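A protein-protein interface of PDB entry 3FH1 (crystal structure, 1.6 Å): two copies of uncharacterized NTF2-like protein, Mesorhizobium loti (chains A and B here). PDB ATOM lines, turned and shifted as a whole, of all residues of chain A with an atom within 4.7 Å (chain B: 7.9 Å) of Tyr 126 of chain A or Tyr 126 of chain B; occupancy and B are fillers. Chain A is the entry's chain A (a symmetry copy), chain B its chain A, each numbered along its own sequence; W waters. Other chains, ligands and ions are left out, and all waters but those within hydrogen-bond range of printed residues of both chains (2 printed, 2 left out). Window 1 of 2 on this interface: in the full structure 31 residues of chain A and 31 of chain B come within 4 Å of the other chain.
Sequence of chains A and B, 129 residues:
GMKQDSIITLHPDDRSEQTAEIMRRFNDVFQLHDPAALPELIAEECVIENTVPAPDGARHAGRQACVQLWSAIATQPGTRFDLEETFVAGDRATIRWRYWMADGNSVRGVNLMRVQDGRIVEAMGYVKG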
ATOM      1  N   THR A  51      11.481 -33.543  21.331  1.00  0.00           N
ATOM      2  CA  THR A  51      11.837 -33.886  19.943  1.00  0.00           C
ATOM      3  C   THR A  51      11.286 -35.198  19.475  1.00  0.00           C
ATOM      4  O   THR A  51      11.146 -35.414  18.271  1.00  0.00           O
ATOM      5  CB  THR A  51      13.349 -33.962  19.780  1.00  0.00           C
ATOM      6  OG1 THR A  51      13.873 -34.922  20.734  1.00  0.00           O
ATOM      7  CG2 THR A  51      14.063 -32.620  19.975  1.00  0.00           C
ATOM      8  N   GLU A  84      24.699 -23.959  16.852  1.00  0.00           N
ATOM      9  CA  GLU A  84      24.810 -23.469  15.490  1.00  0.00           C
ATOM     10  C   GLU A  84      24.431 -21.992  15.407  1.00  0.00           C
ATOM     11  O   GLU A  84      25.164 -21.188  14.814  1.00  0.00           O
ATOM     12  CB  GLU A  84      23.979 -24.294  14.509  1.00  0.00           C
ATOM     13  CG  GLU A  84      24.460 -25.698  14.358  1.00  0.00           C
ATOM     14  CD  GLU A  84      23.602 -26.506  13.364  1.00  0.00           C
ATOM     15  OE1 GLU A  84      22.516 -26.017  12.971  1.00  0.00           O
ATOM     16  OE2 GLU A  84      24.022 -27.613  12.997  1.00  0.00           O
ATOM     17  N   ARG A  96      19.419 -23.245  17.078  1.00  0.00           N
ATOM     18  CA  ARG A  96      19.848 -24.408  16.279  1.00  0.00           C
ATOM     19  C   ARG A  96      21.079 -25.007  16.903  1.00  0.00           C
ATOM     20  O   ARG A  96      22.000 -24.307  17.321  1.00  0.00           O
ATOM     21  CB  ARG A  96      20.100 -24.050  14.808  1.00  0.00           C
ATOM     22  CG  ARG A  96      18.828 -23.869  13.981  1.00  0.00           C
ATOM     23  CD  ARG A  96      19.230 -23.702  12.524  1.00  0.00           C
ATOM     24  NE  ARG A  96      19.952 -22.482  12.154  1.00  0.00           N
ATOM     25  CZ  ARG A  96      21.194 -22.442  11.658  1.00  0.00           C
ATOM     26  NH1 ARG A  96      21.966 -23.498  11.642  1.00  0.00           N
ATOM     27  NH2 ARG A  96      21.700 -21.299  11.200  1.00  0.00           N
ATOM     28  N   TRP A  97      21.112 -26.336  16.922  1.00  0.00           N
ATOM     29  CA  TRP A  97      22.147 -27.124  17.556  1.00  0.00           C
ATOM     30  C   TRP A  97      22.445 -28.433  16.871  1.00  0.00           C
ATOM     31  O   TRP A  97      21.698 -28.906  16.028  1.00  0.00           O
ATOM     32  CB  TRP A  97      21.783 -27.372  19.043  1.00  0.00           C
ATOM     33  CG  TRP A  97      20.386 -27.840  19.286  1.00  0.00           C
ATOM     34  CD1 TRP A  97      19.376 -27.077  19.802  1.00  0.00           C
ATOM     35  CD2 TRP A  97      19.841 -29.171  19.147  1.00  0.00           C
ATOM     36  NE1 TRP A  97      18.233 -27.806  19.926  1.00  0.00           N
ATOM     37  CE2 TRP A  97      18.486 -29.095  19.552  1.00  0.00           C
ATOM     38  CE3 TRP A  97      20.339 -30.394  18.710  1.00  0.00           C
ATOM     39  CZ2 TRP A  97      17.637 -30.206  19.518  1.00  0.00           C
ATOM     40  CZ3 TRP A  97      19.493 -31.477  18.673  1.00  0.00           C
ATOM     41  CH2 TRP A  97      18.188 -31.385  19.094  1.00  0.00           C
ATOM     42  N   ARG A 108      21.331 -33.016  14.030  1.00  0.00           N
ATOM     43  CA  ARG A 108      20.984 -31.601  14.098  1.00  0.00           C
ATOM     44  C   ARG A 108      19.547 -31.401  14.528  1.00  0.00           C
ATOM     45  O   ARG A 108      18.657 -32.193  14.202  1.00  0.00           O
ATOM     46  CB  ARG A 108      21.246 -30.933  12.761  1.00  0.00           C
ATOM     47  CG  ARG A 108      22.644 -31.020  12.221  1.00  0.00           C
ATOM     48  CD  ARG A 108      22.751 -30.349  10.873  1.00  0.00           C
ATOM     49  NE  ARG A 108      22.639 -28.896  10.937  1.00  0.00           N
ATOM     50  CZ  ARG A 108      22.159 -28.149   9.945  1.00  0.00           C
ATOM     51  NH1 ARG A 108      21.775 -28.696   8.820  1.00  0.00           N
ATOM     52  NH2 ARG A 108      22.094 -26.838  10.078  1.00  0.00           N
ATOM     53  N   GLY A 109      19.310 -30.291  15.218  1.00  0.00           N
ATOM     54  CA  GLY A 109      17.973 -29.944  15.731  1.00  0.00           C
ATOM     55  C   GLY A 109      17.813 -28.489  16.007  1.00  0.00           C
ATOM     56  O   GLY A 109      18.706 -27.661  15.754  1.00  0.00           O
ATOM     57  N   VAL A 110      16.648 -28.152  16.532  1.00  0.00           N
ATOM     58  CA  VAL A 110      16.320 -26.790  16.829  1.00  0.00           C
ATOM     59  C   VAL A 110      15.325 -26.765  17.983  1.00  0.00           C
ATOM     60  O   VAL A 110      14.471 -27.676  18.135  1.00  0.00           O
ATOM     61  CB  VAL A 110      15.678 -26.060  15.589  1.00  0.00           C
ATOM     62  CG1 VAL A 110      14.344 -26.705  15.172  1.00  0.00           C
ATOM     63  CG2 VAL A 110      15.611 -24.525  15.841  1.00  0.00           C
ATOM     64  N   MET A 124       9.993 -25.900  22.345  1.00  0.00           N
ATOM     65  CA  MET A 124       9.512 -26.890  21.356  1.00  0.00           C
ATOM     66  C   MET A 124      10.667 -27.396  20.502  1.00  0.00           C
ATOM     67  O   MET A 124      11.269 -26.642  19.741  1.00  0.00           O
ATOM     68  CB  MET A 124       8.411 -26.252  20.492  1.00  0.00           C
ATOM     69  CG  MET A 124       7.268 -25.701  21.301  1.00  0.00           C
ATOM     70  SD  MET A 124       6.084 -24.777  20.148  1.00  0.00           S
ATOM     71  CE  MET A 124       4.520 -24.796  21.101  1.00  0.00           C
ATOM     72  N   GLY A 125      10.988 -28.670  20.646  1.00  0.00           N
ATOM     73  CA  GLY A 125      12.158 -29.248  20.018  1.00  0.00           C
ATOM     74  C   GLY A 125      11.867 -30.096  18.809  1.00  0.00           C
ATOM     75  O   GLY A 125      10.875 -30.838  18.753  1.00  0.00           O
ATOM     76  N   TYR A 126      12.748 -29.959  17.788  1.00  0.00           N
ATOM     77  CA  TYR A 126      12.663 -30.755  16.574  1.00  0.00           C
ATOM     78  C   TYR A 126      14.046 -31.187  16.084  1.00  0.00           C
ATOM     79  O   TYR A 126      15.027 -30.556  16.454  1.00  0.00           O
ATOM     80  CB  TYR A 126      11.995 -29.966  15.468  1.00  0.00           C
ATOM     81  CG  TYR A 126      10.618 -29.385  15.788  1.00  0.00           C
ATOM     82  CD1 TYR A 126      10.484 -28.261  16.565  1.00  0.00           C
ATOM     83  CD2 TYR A 126       9.469 -29.982  15.330  1.00  0.00           C
ATOM     84  CE1 TYR A 126       9.226 -27.709  16.820  1.00  0.00           C
ATOM     85  CE2 TYR A 126       8.215 -29.448  15.595  1.00  0.00           C
ATOM     86  CZ  TYR A 126       8.088 -28.316  16.367  1.00  0.00           C
ATOM     87  OH  TYR A 126       6.835 -27.768  16.637  1.00  0.00           O
ATOM     88  N   VAL A 127      14.101 -32.215  15.234  1.00  0.00           N
ATOM     89  CA  VAL A 127      15.338 -32.795  14.763  1.00  0.00           C
ATOM     90  C   VAL A 127      15.261 -33.124  13.297  1.00  0.00           C
ATOM     91  O   VAL A 127      14.194 -33.124  12.717  1.00  0.00           O
ATOM     92  CB  VAL A 127      15.693 -34.092  15.529  1.00  0.00           C
ATOM     93  CG1 VAL A 127      16.142 -33.761  16.955  1.00  0.00           C
ATOM     94  CG2 VAL A 127      14.515 -35.103  15.534  1.00  0.00           C
ATOM     95  N   LYS A 128      16.393 -33.436  12.685  1.00  0.00           N
ATOM     96  CA  LYS A 128      16.364 -34.107  11.384  1.00  0.00           C
ATOM     97  C   LYS A 128      15.926 -35.518  11.644  1.00  0.00           C
ATOM     98  O   LYS A 128      16.325 -36.126  12.649  1.00  0.00           O
ATOM     99  CB  LYS A 128      17.760 -34.099  10.760  1.00  0.00           C
ATOM    100  CG  LYS A 128      18.312 -32.679  10.565  1.00  0.00           C
ATOM    101  CD  LYS A 128      17.401 -31.805   9.661  1.00  0.00           C
ATOM    102  CE  LYS A 128      18.025 -30.428   9.322  1.00  0.00           C
ATOM    103  NZ  LYS A 128      17.151 -29.532   8.474  1.00  0.00           N
ATOM    104  N   GLU B  49      17.508 -26.870   3.620  1.00  0.00           N
ATOM    105  CA  GLU B  49      18.104 -27.946   4.417  1.00  0.00           C
ATOM    106  C   GLU B  49      16.893 -28.760   4.797  1.00  0.00           C
ATOM    107  O   GLU B  49      16.103 -28.375   5.649  1.00  0.00           O
ATOM    108  CB  GLU B  49      18.877 -27.411   5.593  1.00  0.00           C
ATOM    109  CG  GLU B  49      20.094 -26.601   5.153  1.00  0.00           C
ATOM    110  CD  GLU B  49      21.003 -26.179   6.272  1.00  0.00           C
ATOM    111  OE1 GLU B  49      20.690 -26.405   7.461  1.00  0.00           O
ATOM    112  OE2 GLU B  49      22.060 -25.565   5.931  1.00  0.00           O
ATOM    113  N   ASN B  50      16.668 -29.872   4.102  1.00  0.00           N
ATOM    114  CA  ASN B  50      15.422 -30.618   4.296  1.00  0.00           C
ATOM    115  C   ASN B  50      15.439 -31.407   5.613  1.00  0.00           C
ATOM    116  O   ASN B  50      16.467 -31.617   6.255  1.00  0.00           O
ATOM    117  CB  ASN B  50      15.123 -31.541   3.096  1.00  0.00           C
ATOM    118  CG  ASN B  50      13.599 -31.910   2.924  1.00  0.00           C
ATOM    119  OD1 ASN B  50      12.682 -31.364   3.556  1.00  0.00           O
ATOM    120  ND2 ASN B  50      13.360 -32.863   2.015  1.00  0.00           N
ATOM    121  N   THR B  51      14.262 -31.906   5.941  1.00  0.00           N
ATOM    122  CA  THR B  51      13.958 -32.543   7.234  1.00  0.00           C
ATOM    123  C   THR B  51      14.649 -33.854   7.448  1.00  0.00           C
ATOM    124  O   THR B  51      14.823 -34.281   8.590  1.00  0.00           O
ATOM    125  CB  THR B  51      12.464 -32.808   7.363  1.00  0.00           C
ATOM    126  OG1 THR B  51      12.035 -33.618   6.238  1.00  0.00           O
ATOM    127  CG2 THR B  51      11.610 -31.536   7.422  1.00  0.00           C
ATOM    128  N   VAL B  52      15.001 -34.492   6.339  1.00  0.00           N
ATOM    129  CA  VAL B  52      15.622 -35.805   6.318  1.00  0.00           C
ATOM    130  C   VAL B  52      16.725 -35.878   5.283  1.00  0.00           C
ATOM    131  O   VAL B  52      16.752 -35.114   4.321  1.00  0.00           O
ATOM    132  CB  VAL B  52      14.566 -36.929   5.993  1.00  0.00           C
ATOM    133  CG1 VAL B  52      13.510 -36.931   7.070  1.00  0.00           C
ATOM    134  CG2 VAL B  52      13.895 -36.698   4.620  1.00  0.00           C
ATOM    135  N   PRO B  55      22.023 -37.429   9.903  1.00  0.00           N
ATOM    136  CA  PRO B  55      22.162 -36.351  10.866  1.00  0.00           C
ATOM    137  C   PRO B  55      21.909 -34.971  10.393  1.00  0.00           C
ATOM    138  O   PRO B  55      21.495 -34.142  11.202  1.00  0.00           O
ATOM    139  CB  PRO B  55      23.614 -36.470  11.286  1.00  0.00           C
ATOM    140  CG  PRO B  55      24.308 -37.012  10.076  1.00  0.00           C
ATOM    141  CD  PRO B  55      23.341 -37.990   9.499  1.00  0.00           C
ATOM    142  N   ASP B  56      22.137 -34.696   9.119  1.00  0.00           N
ATOM    143  CA  ASP B  56      22.242 -33.311   8.634  1.00  0.00           C
ATOM    144  C   ASP B  56      21.046 -32.715   7.907  1.00  0.00           C
ATOM    145  O   ASP B  56      20.902 -31.478   7.791  1.00  0.00           O
ATOM    146  CB  ASP B  56      23.463 -33.185   7.712  1.00  0.00           C
ATOM    147  CG  ASP B  56      24.755 -33.391   8.412  1.00  0.00           C
ATOM    148  OD1 ASP B  56      24.865 -32.972   9.574  1.00  0.00           O
ATOM    149  OD2 ASP B  56      25.685 -34.004   7.838  1.00  0.00           O
ATOM    150  N   GLY B  57      20.226 -33.604   7.339  1.00  0.00           N
ATOM    151  CA  GLY B  57      19.220 -33.250   6.379  1.00  0.00           C
ATOM    152  C   GLY B  57      19.875 -33.080   5.011  1.00  0.00           C
ATOM    153  O   GLY B  57      20.991 -32.588   4.951  1.00  0.00           O
ATOM    154  N   GLU B  84       0.154 -24.801  12.035  1.00  0.00           N
ATOM    155  CA  GLU B  84       0.006 -24.596  13.464  1.00  0.00           C
ATOM    156  C   GLU B  84       0.228 -23.130  13.832  1.00  0.00           C
ATOM    157  O   GLU B  84      -0.580 -22.536  14.559  1.00  0.00           O
ATOM    158  CB  GLU B  84       0.929 -25.501  14.277  1.00  0.00           C
ATOM    159  CG  GLU B  84       0.600 -26.950  14.152  1.00  0.00           C
ATOM    160  CD  GLU B  84       1.549 -27.838  14.982  1.00  0.00           C
ATOM    161  OE1 GLU B  84       2.581 -27.322  15.472  1.00  0.00           O
ATOM    162  OE2 GLU B  84       1.252 -29.034  15.126  1.00  0.00           O
ATOM    163  N   ILE B  95       7.553 -21.462  10.758  1.00  0.00           N
ATOM    164  CA  ILE B  95       6.237 -22.000  10.379  1.00  0.00           C
ATOM    165  C   ILE B  95       6.155 -23.372  10.959  1.00  0.00           C
ATOM    166  O   ILE B  95       6.897 -24.280  10.531  1.00  0.00           O
ATOM    167  CB  ILE B  95       6.025 -22.118   8.846  1.00  0.00           C
ATOM    168  CG1 ILE B  95       6.352 -20.776   8.142  1.00  0.00           C
ATOM    169  CG2 ILE B  95       4.633 -22.596   8.573  1.00  0.00           C
ATOM    170  CD1 ILE B  95       6.527 -20.933   6.598  1.00  0.00           C
ATOM    171  N   ARG B  96       5.327 -23.506  12.003  1.00  0.00           N
ATOM    172  CA  ARG B  96       5.031 -24.838  12.561  1.00  0.00           C
ATOM    173  C   ARG B  96       3.863 -25.434  11.821  1.00  0.00           C
ATOM    174  O   ARG B  96       2.869 -24.767  11.535  1.00  0.00           O
ATOM    175  CB  ARG B  96       4.758 -24.797  14.070  1.00  0.00           C
ATOM    176  CG  ARG B  96       6.012 -24.644  14.929  1.00  0.00           C
ATOM    177  CD  ARG B  96       5.609 -24.802  16.387  1.00  0.00           C
ATOM    178  NE  ARG B  96       4.766 -23.759  16.976  1.00  0.00           N
ATOM    179  CZ  ARG B  96       3.532 -23.945  17.458  1.00  0.00           C
ATOM    180  NH1 ARG B  96       2.876 -25.060  17.264  1.00  0.00           N
ATOM    181  NH2 ARG B  96       2.913 -22.970  18.121  1.00  0.00           N
ATOM    182  N   TRP B  97       3.971 -26.730  11.548  1.00  0.00           N
ATOM    183  CA  TRP B  97       3.017 -27.487  10.764  1.00  0.00           C
ATOM    184  C   TRP B  97       2.866 -28.927  11.183  1.00  0.00           C
ATOM    185  O   TRP B  97       3.668 -29.471  11.927  1.00  0.00           O
ATOM    186  CB  TRP B  97       3.391 -27.407   9.261  1.00  0.00           C
ATOM    187  CG  TRP B  97       4.826 -27.670   8.948  1.00  0.00           C
ATOM    188  CD1 TRP B  97       5.745 -26.720   8.597  1.00  0.00           C
ATOM    189  CD2 TRP B  97       5.510 -28.937   8.835  1.00  0.00           C
ATOM    190  NE1 TRP B  97       6.957 -27.287   8.347  1.00  0.00           N
ATOM    191  CE2 TRP B  97       6.846 -28.643   8.465  1.00  0.00           C
ATOM    192  CE3 TRP B  97       5.149 -30.266   9.025  1.00  0.00           C
ATOM    193  CZ2 TRP B  97       7.807 -29.644   8.295  1.00  0.00           C
ATOM    194  CZ3 TRP B  97       6.104 -31.242   8.862  1.00  0.00           C
ATOM    195  CH2 TRP B  97       7.388 -30.934   8.481  1.00  0.00           C
ATOM    196  N   VAL B 107       3.028 -36.193  10.920  1.00  0.00           N
ATOM    197  CA  VAL B 107       4.173 -35.822  11.723  1.00  0.00           C
ATOM    198  C   VAL B 107       4.189 -34.288  11.897  1.00  0.00           C
ATOM    199  O   VAL B 107       3.883 -33.528  10.975  1.00  0.00           O
ATOM    200  CB  VAL B 107       5.522 -36.340  11.147  1.00  0.00           C
ATOM    201  CG1 VAL B 107       5.808 -35.759   9.730  1.00  0.00           C
ATOM    202  CG2 VAL B 107       6.678 -36.056  12.126  1.00  0.00           C
ATOM    203  N   ARG B 108       4.486 -33.825  13.107  1.00  0.00           N
ATOM    204  CA  ARG B 108       4.681 -32.395  13.314  1.00  0.00           C
ATOM    205  C   ARG B 108       6.085 -31.966  12.945  1.00  0.00           C
ATOM    206  O   ARG B 108       7.057 -32.707  13.123  1.00  0.00           O
ATOM    207  CB  ARG B 108       4.364 -32.026  14.751  1.00  0.00           C
ATOM    208  CG  ARG B 108       2.989 -32.361  15.251  1.00  0.00           C
ATOM    209  CD  ARG B 108       2.825 -31.975  16.701  1.00  0.00           C
ATOM    210  NE  ARG B 108       2.782 -30.533  16.917  1.00  0.00           N
ATOM    211  CZ  ARG B 108       3.191 -29.943  18.038  1.00  0.00           C
ATOM    212  NH1 ARG B 108       3.643 -30.652  19.042  1.00  0.00           N
ATOM    213  NH2 ARG B 108       3.116 -28.632  18.159  1.00  0.00           N
ATOM    214  N   GLY B 109       6.196 -30.725  12.483  1.00  0.00           N
ATOM    215  CA  GLY B 109       7.484 -30.148  12.059  1.00  0.00           C
ATOM    216  C   GLY B 109       7.487 -28.658  12.068  1.00  0.00           C
ATOM    217  O   GLY B 109       6.514 -27.993  12.465  1.00  0.00           O
ATOM    218  N   VAL B 110       8.605 -28.107  11.628  1.00  0.00           N
ATOM    219  CA  VAL B 110       8.785 -26.686  11.602  1.00  0.00           C
ATOM    220  C   VAL B 110       9.759 -26.336  10.484  1.00  0.00           C
ATOM    221  O   VAL B 110      10.703 -27.106  10.169  1.00  0.00           O
ATOM    222  CB  VAL B 110       9.358 -26.143  12.964  1.00  0.00           C
ATOM    223  CG1 VAL B 110      10.757 -26.712  13.264  1.00  0.00           C
ATOM    224  CG2 VAL B 110       9.261 -24.590  13.011  1.00  0.00           C
ATOM    225  N   ASN B 111       9.507 -25.181   9.867  1.00  0.00           N
ATOM    226  CA  ASN B 111      10.445 -24.578   8.941  1.00  0.00           C
ATOM    227  C   ASN B 111      10.984 -23.262   9.553  1.00  0.00           C
ATOM    228  O   ASN B 111      10.213 -22.434  10.095  1.00  0.00           O
ATOM    229  CB  ASN B 111       9.789 -24.112   7.636  1.00  0.00           C
ATOM    230  CG  ASN B 111       9.450 -25.224   6.701  1.00  0.00           C
ATOM    231  OD1 ASN B 111       9.384 -26.375   7.062  1.00  0.00           O
ATOM    232  ND2 ASN B 111       9.271 -24.867   5.419  1.00  0.00           N
ATOM    233  N   LEU B 112      12.306 -23.080   9.493  1.00  0.00           N
ATOM    234  CA  LEU B 112      12.938 -21.806   9.777  1.00  0.00           C
ATOM    235  C   LEU B 112      13.289 -21.144   8.454  1.00  0.00           C
ATOM    236  O   LEU B 112      14.092 -21.646   7.654  1.00  0.00           O
ATOM    237  CB  LEU B 112      14.220 -21.950  10.586  1.00  0.00           C
ATOM    238  CG  LEU B 112      14.073 -21.924  12.100  1.00  0.00           C
ATOM    239  CD1 LEU B 112      13.171 -23.118  12.560  1.00  0.00           C
ATOM    240  CD2 LEU B 112      15.473 -21.934  12.780  1.00  0.00           C
ATOM    241  N   ALA B 123      15.689 -22.013   3.835  1.00  0.00           N
ATOM    242  CA  ALA B 123      14.564 -22.717   4.454  1.00  0.00           C
ATOM    243  C   ALA B 123      15.152 -23.950   5.116  1.00  0.00           C
ATOM    244  O   ALA B 123      15.762 -24.797   4.432  1.00  0.00           O
ATOM    245  CB  ALA B 123      13.510 -23.144   3.442  1.00  0.00           C
ATOM    246  N   MET B 124      14.926 -24.096   6.421  1.00  0.00           N
ATOM    247  CA  MET B 124      15.518 -25.201   7.208  1.00  0.00           C
ATOM    248  C   MET B 124      14.432 -25.979   7.938  1.00  0.00           C
ATOM    249  O   MET B 124      13.761 -25.452   8.822  1.00  0.00           O
ATOM    250  CB  MET B 124      16.555 -24.627   8.190  1.00  0.00           C
ATOM    251  CG  MET B 124      17.625 -23.815   7.512  1.00  0.00           C
ATOM    252  SD  MET B 124      18.717 -23.009   8.832  1.00  0.00           S
ATOM    253  CE  MET B 124      20.265 -22.680   7.910  1.00  0.00           C
ATOM    254  N   GLY B 125      14.245 -27.229   7.549  1.00  0.00           N
ATOM    255  CA  GLY B 125      13.149 -28.037   8.043  1.00  0.00           C
ATOM    256  C   GLY B 125      13.540 -29.064   9.071  1.00  0.00           C
ATOM    257  O   GLY B 125      14.605 -29.695   8.994  1.00  0.00           O
ATOM    258  N   TYR B 126      12.661 -29.219  10.090  1.00  0.00           N
ATOM    259  CA  TYR B 126      12.841 -30.219  11.130  1.00  0.00           C
ATOM    260  C   TYR B 126      11.516 -30.880  11.514  1.00  0.00           C
ATOM    261  O   TYR B 126      10.470 -30.297  11.262  1.00  0.00           O
ATOM    262  CB  TYR B 126      13.433 -29.590  12.373  1.00  0.00           C
ATOM    263  CG  TYR B 126      14.738 -28.817  12.184  1.00  0.00           C
ATOM    264  CD1 TYR B 126      14.745 -27.557  11.639  1.00  0.00           C
ATOM    265  CD2 TYR B 126      15.949 -29.366  12.532  1.00  0.00           C
ATOM    266  CE1 TYR B 126      15.936 -26.837  11.506  1.00  0.00           C
ATOM    267  CE2 TYR B 126      17.136 -28.662  12.387  1.00  0.00           C
ATOM    268  CZ  TYR B 126      17.135 -27.396  11.847  1.00  0.00           C
ATOM    269  OH  TYR B 126      18.321 -26.678  11.699  1.00  0.00           O
ATOM    270  N   VAL B 127      11.579 -32.052  12.151  1.00  0.00           N
ATOM    271  CA  VAL B 127      10.414 -32.837  12.491  1.00  0.00           C
ATOM    272  C   VAL B 127      10.540 -33.431  13.868  1.00  0.00           C
ATOM    273  O   VAL B 127      11.607 -33.430  14.447  1.00  0.00           O
ATOM    274  CB  VAL B 127      10.190 -33.994  11.487  1.00  0.00           C
ATOM    275  CG1 VAL B 127       9.694 -33.446  10.146  1.00  0.00           C
ATOM    276  CG2 VAL B 127      11.468 -34.856  11.301  1.00  0.00           C
ATOM    277  N   LYS B 128       9.454 -33.971  14.397  1.00  0.00           N
ATOM    278  CA  LYS B 128       9.567 -34.872  15.546  1.00  0.00           C
ATOM    279  C   LYS B 128      10.149 -36.153  15.026  1.00  0.00           C
ATOM    280  O   LYS B 128       9.805 -36.596  13.918  1.00  0.00           O
ATOM    281  CB  LYS B 128       8.184 -35.131  16.145  1.00  0.00           C
ATOM    282  CG  LYS B 128       7.488 -33.841  16.603  1.00  0.00           C
ATOM    283  CD  LYS B 128       8.311 -33.065  17.666  1.00  0.00           C
ATOM    284  CE  LYS B 128       7.549 -31.851  18.256  1.00  0.00           C
ATOM    285  NZ  LYS B 128       8.332 -31.047  19.269  1.00  0.00           N
ATOM    286  N   GLY B 129      11.018 -36.757  15.819  1.00  0.00           N
ATOM    287  CA  GLY B 129      11.788 -37.899  15.361  1.00  0.00           C
ATOM    288  C   GLY B 129      11.351 -39.228  15.894  1.00  0.00           C
ATOM    289  O   GLY B 129      12.083 -40.165  15.546  1.00  0.00           O
ATOM    290  OXT GLY B 129      10.381 -39.429  16.656  1.00  0.00           O
HETATM  291  O   HOH W   1       6.649 -28.893  19.245  1.00  0.00           O
HETATM  292  O   HOH W   2      18.597 -27.258   8.926  1.00  0.00           O
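Arg 96 of chain A touches Met 124 of chain B, and with the chains exchanged Met 124 of chain A touches Arg 96 of chain B.
Of the 28 pairs that touch across the chains among the printed residues, 18 have their exchanged pair printed and touching as well.
SD of Met 124 of chain A is in hydrogen-bond range of NE of Arg 96 of chain B (3.6 Å).
The backbone carbonyl oxygen (O) of Asn 50 of chain B is in hydrogen-bond range of the side-chain amino group (NZ) of Lys 128 of chain A (3.1 Å).
N of Val 127 of chain B lies within hydrogen-bond range of O of Val 127 of chain A, at 2.9 Å.
The side-chain amino group (NZ) of Lys 128 of chain A sits at hydrogen-bond distance from the backbone carbonyl oxygen (O) of Glu 49 of chain B (3.2 Å).
The backbone carbonyl oxygen of Thr 51 of chain A lies within hydrogen-bond range of the backbone NH of Gly 129 of chain B, at 2.8 Å.
The backbone NH of Arg 108 of chain A lies within hydrogen-bond range of the backbone carbonyl oxygen of Pro 55 of chain B, 3.0 Å away.
O of Asp 56 of chain B lies within hydrogen-bond range of NH1 of Arg 108 of chain A (3.1 Å).
The side-chain amino group (NZ) of Lys 128 of chain B is in hydrogen-bond range of the backbone carbonyl oxygen (O) of Gly 125 of chain A.
NE of Arg 96 of chain A is in hydrogen-bond range of SD of Met 124 of chain B, at 3.6 Å.
The backbone carbonyl oxygen of Gly 125 of chain B lies within hydrogen-bond range of the side-chain amino group of Lys 128 of chain A, 2.6 Å away.
NH1 of Arg 108 of chain A is in salt-bridge range of OE1 of Glu 49 of chain B (2.9 Å).
Water W2 lies within hydrogen-bond range of the side-chain carboxylate of Glu 49 of chain B (2.7 Å), the side-chain amino group of Lys 128 of chain A (2.7 Å), the side-chain hydroxyl of Tyr 126 of chain B (2.8 Å) and the guanidinium group of Arg 108 of chain A (3.5 Å).
OE1 of Glu 84 of chain A is in salt-bridge range of NH1 of Arg 96 of chain A, 2.9 Å away.
The guanidinium group of Arg 96 of chain B is in salt-bridge range of the side-chain carboxylate of Glu 84 of chain B (2.9 Å).
Printed residues of chain B that touch a printed residue of chain A: Glu 49, Asn 50, Thr 51, Pro 55, Asp 56, Gly 57, Arg 96, Gly 109, Val 110, Met 124, Gly 125, Tyr 126, Val 127, Lys 128 and Gly 129.
Hydrophobic or aromatic side chains of chain B that line the printed part of chain A: Val 110, Met 124, Tyr 126 and Val 127.
Hydrophobic or aromatic side chains of chain A within 4 Å of the printed part of chain B: Val 110, Met 124, Tyr 126 and Val 127.
Of chain A, only Arg 96, Gly 109, Val 110, Tyr 126, Val 127 and Lys 128 come within 4 Å of Tyr 126 of chain B.
Of the printed residues of chain A, Val 110 of chain B touches Tyr 126.
Printed residues of chain B within 4 Å of Val 127 of chain A: Tyr 126 (3.6 Å), Val 127 (2.9 Å) and Gly 129 (3.9 Å).
Of the printed residues of chain A, Val 127 of chain B touches Tyr 126 and Val 127.
Leu 112 of chain B touches none of the printed residues of chain A.
Among the printed residues, pairs that only touch across the chains: Thr 51 of chain A with Lys 128 of chain B (3.2 Å), Arg 96 of chain A with Tyr 126 of chain B (3.2 Å), Gly 109 of chain A with Tyr 126 of chain B (3.7 Å), Val 110 of chain A with Tyr 126 of chain B (3.7 Å), Tyr 126 of chain A with Arg 96 of chain B (3.2 Å), Tyr 126 of chain A with Gly 109 of chain B (3.7 Å), Tyr 126 of chain A with Val 110 of chain B (3.7 Å), Tyr 126 of chain A with Tyr 126 of chain B (3.4 Å), Tyr 126 of chain A with Val 127 of chain B (3.6 Å), Tyr 126 of chain A with Lys 128 of chain B (3.6 Å), Val 127 of chain A with Tyr 126 of chain B (3.6 Å), Val 127 of chain A with Gly 129 of chain B (3.9 Å), Lys 128 of chain A with Thr 51 of chain B (3.2 Å), Lys 128 of chain A with Pro 55 of chain B (3.6 Å), Lys 128 of chain A with Asp 56 of chain B (3.4 Å), Lys 128 of chain A with Gly 57 of chain B (3.9 Å) and Lys 128 of chain A with Tyr 126 of chain B (3.6 Å).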
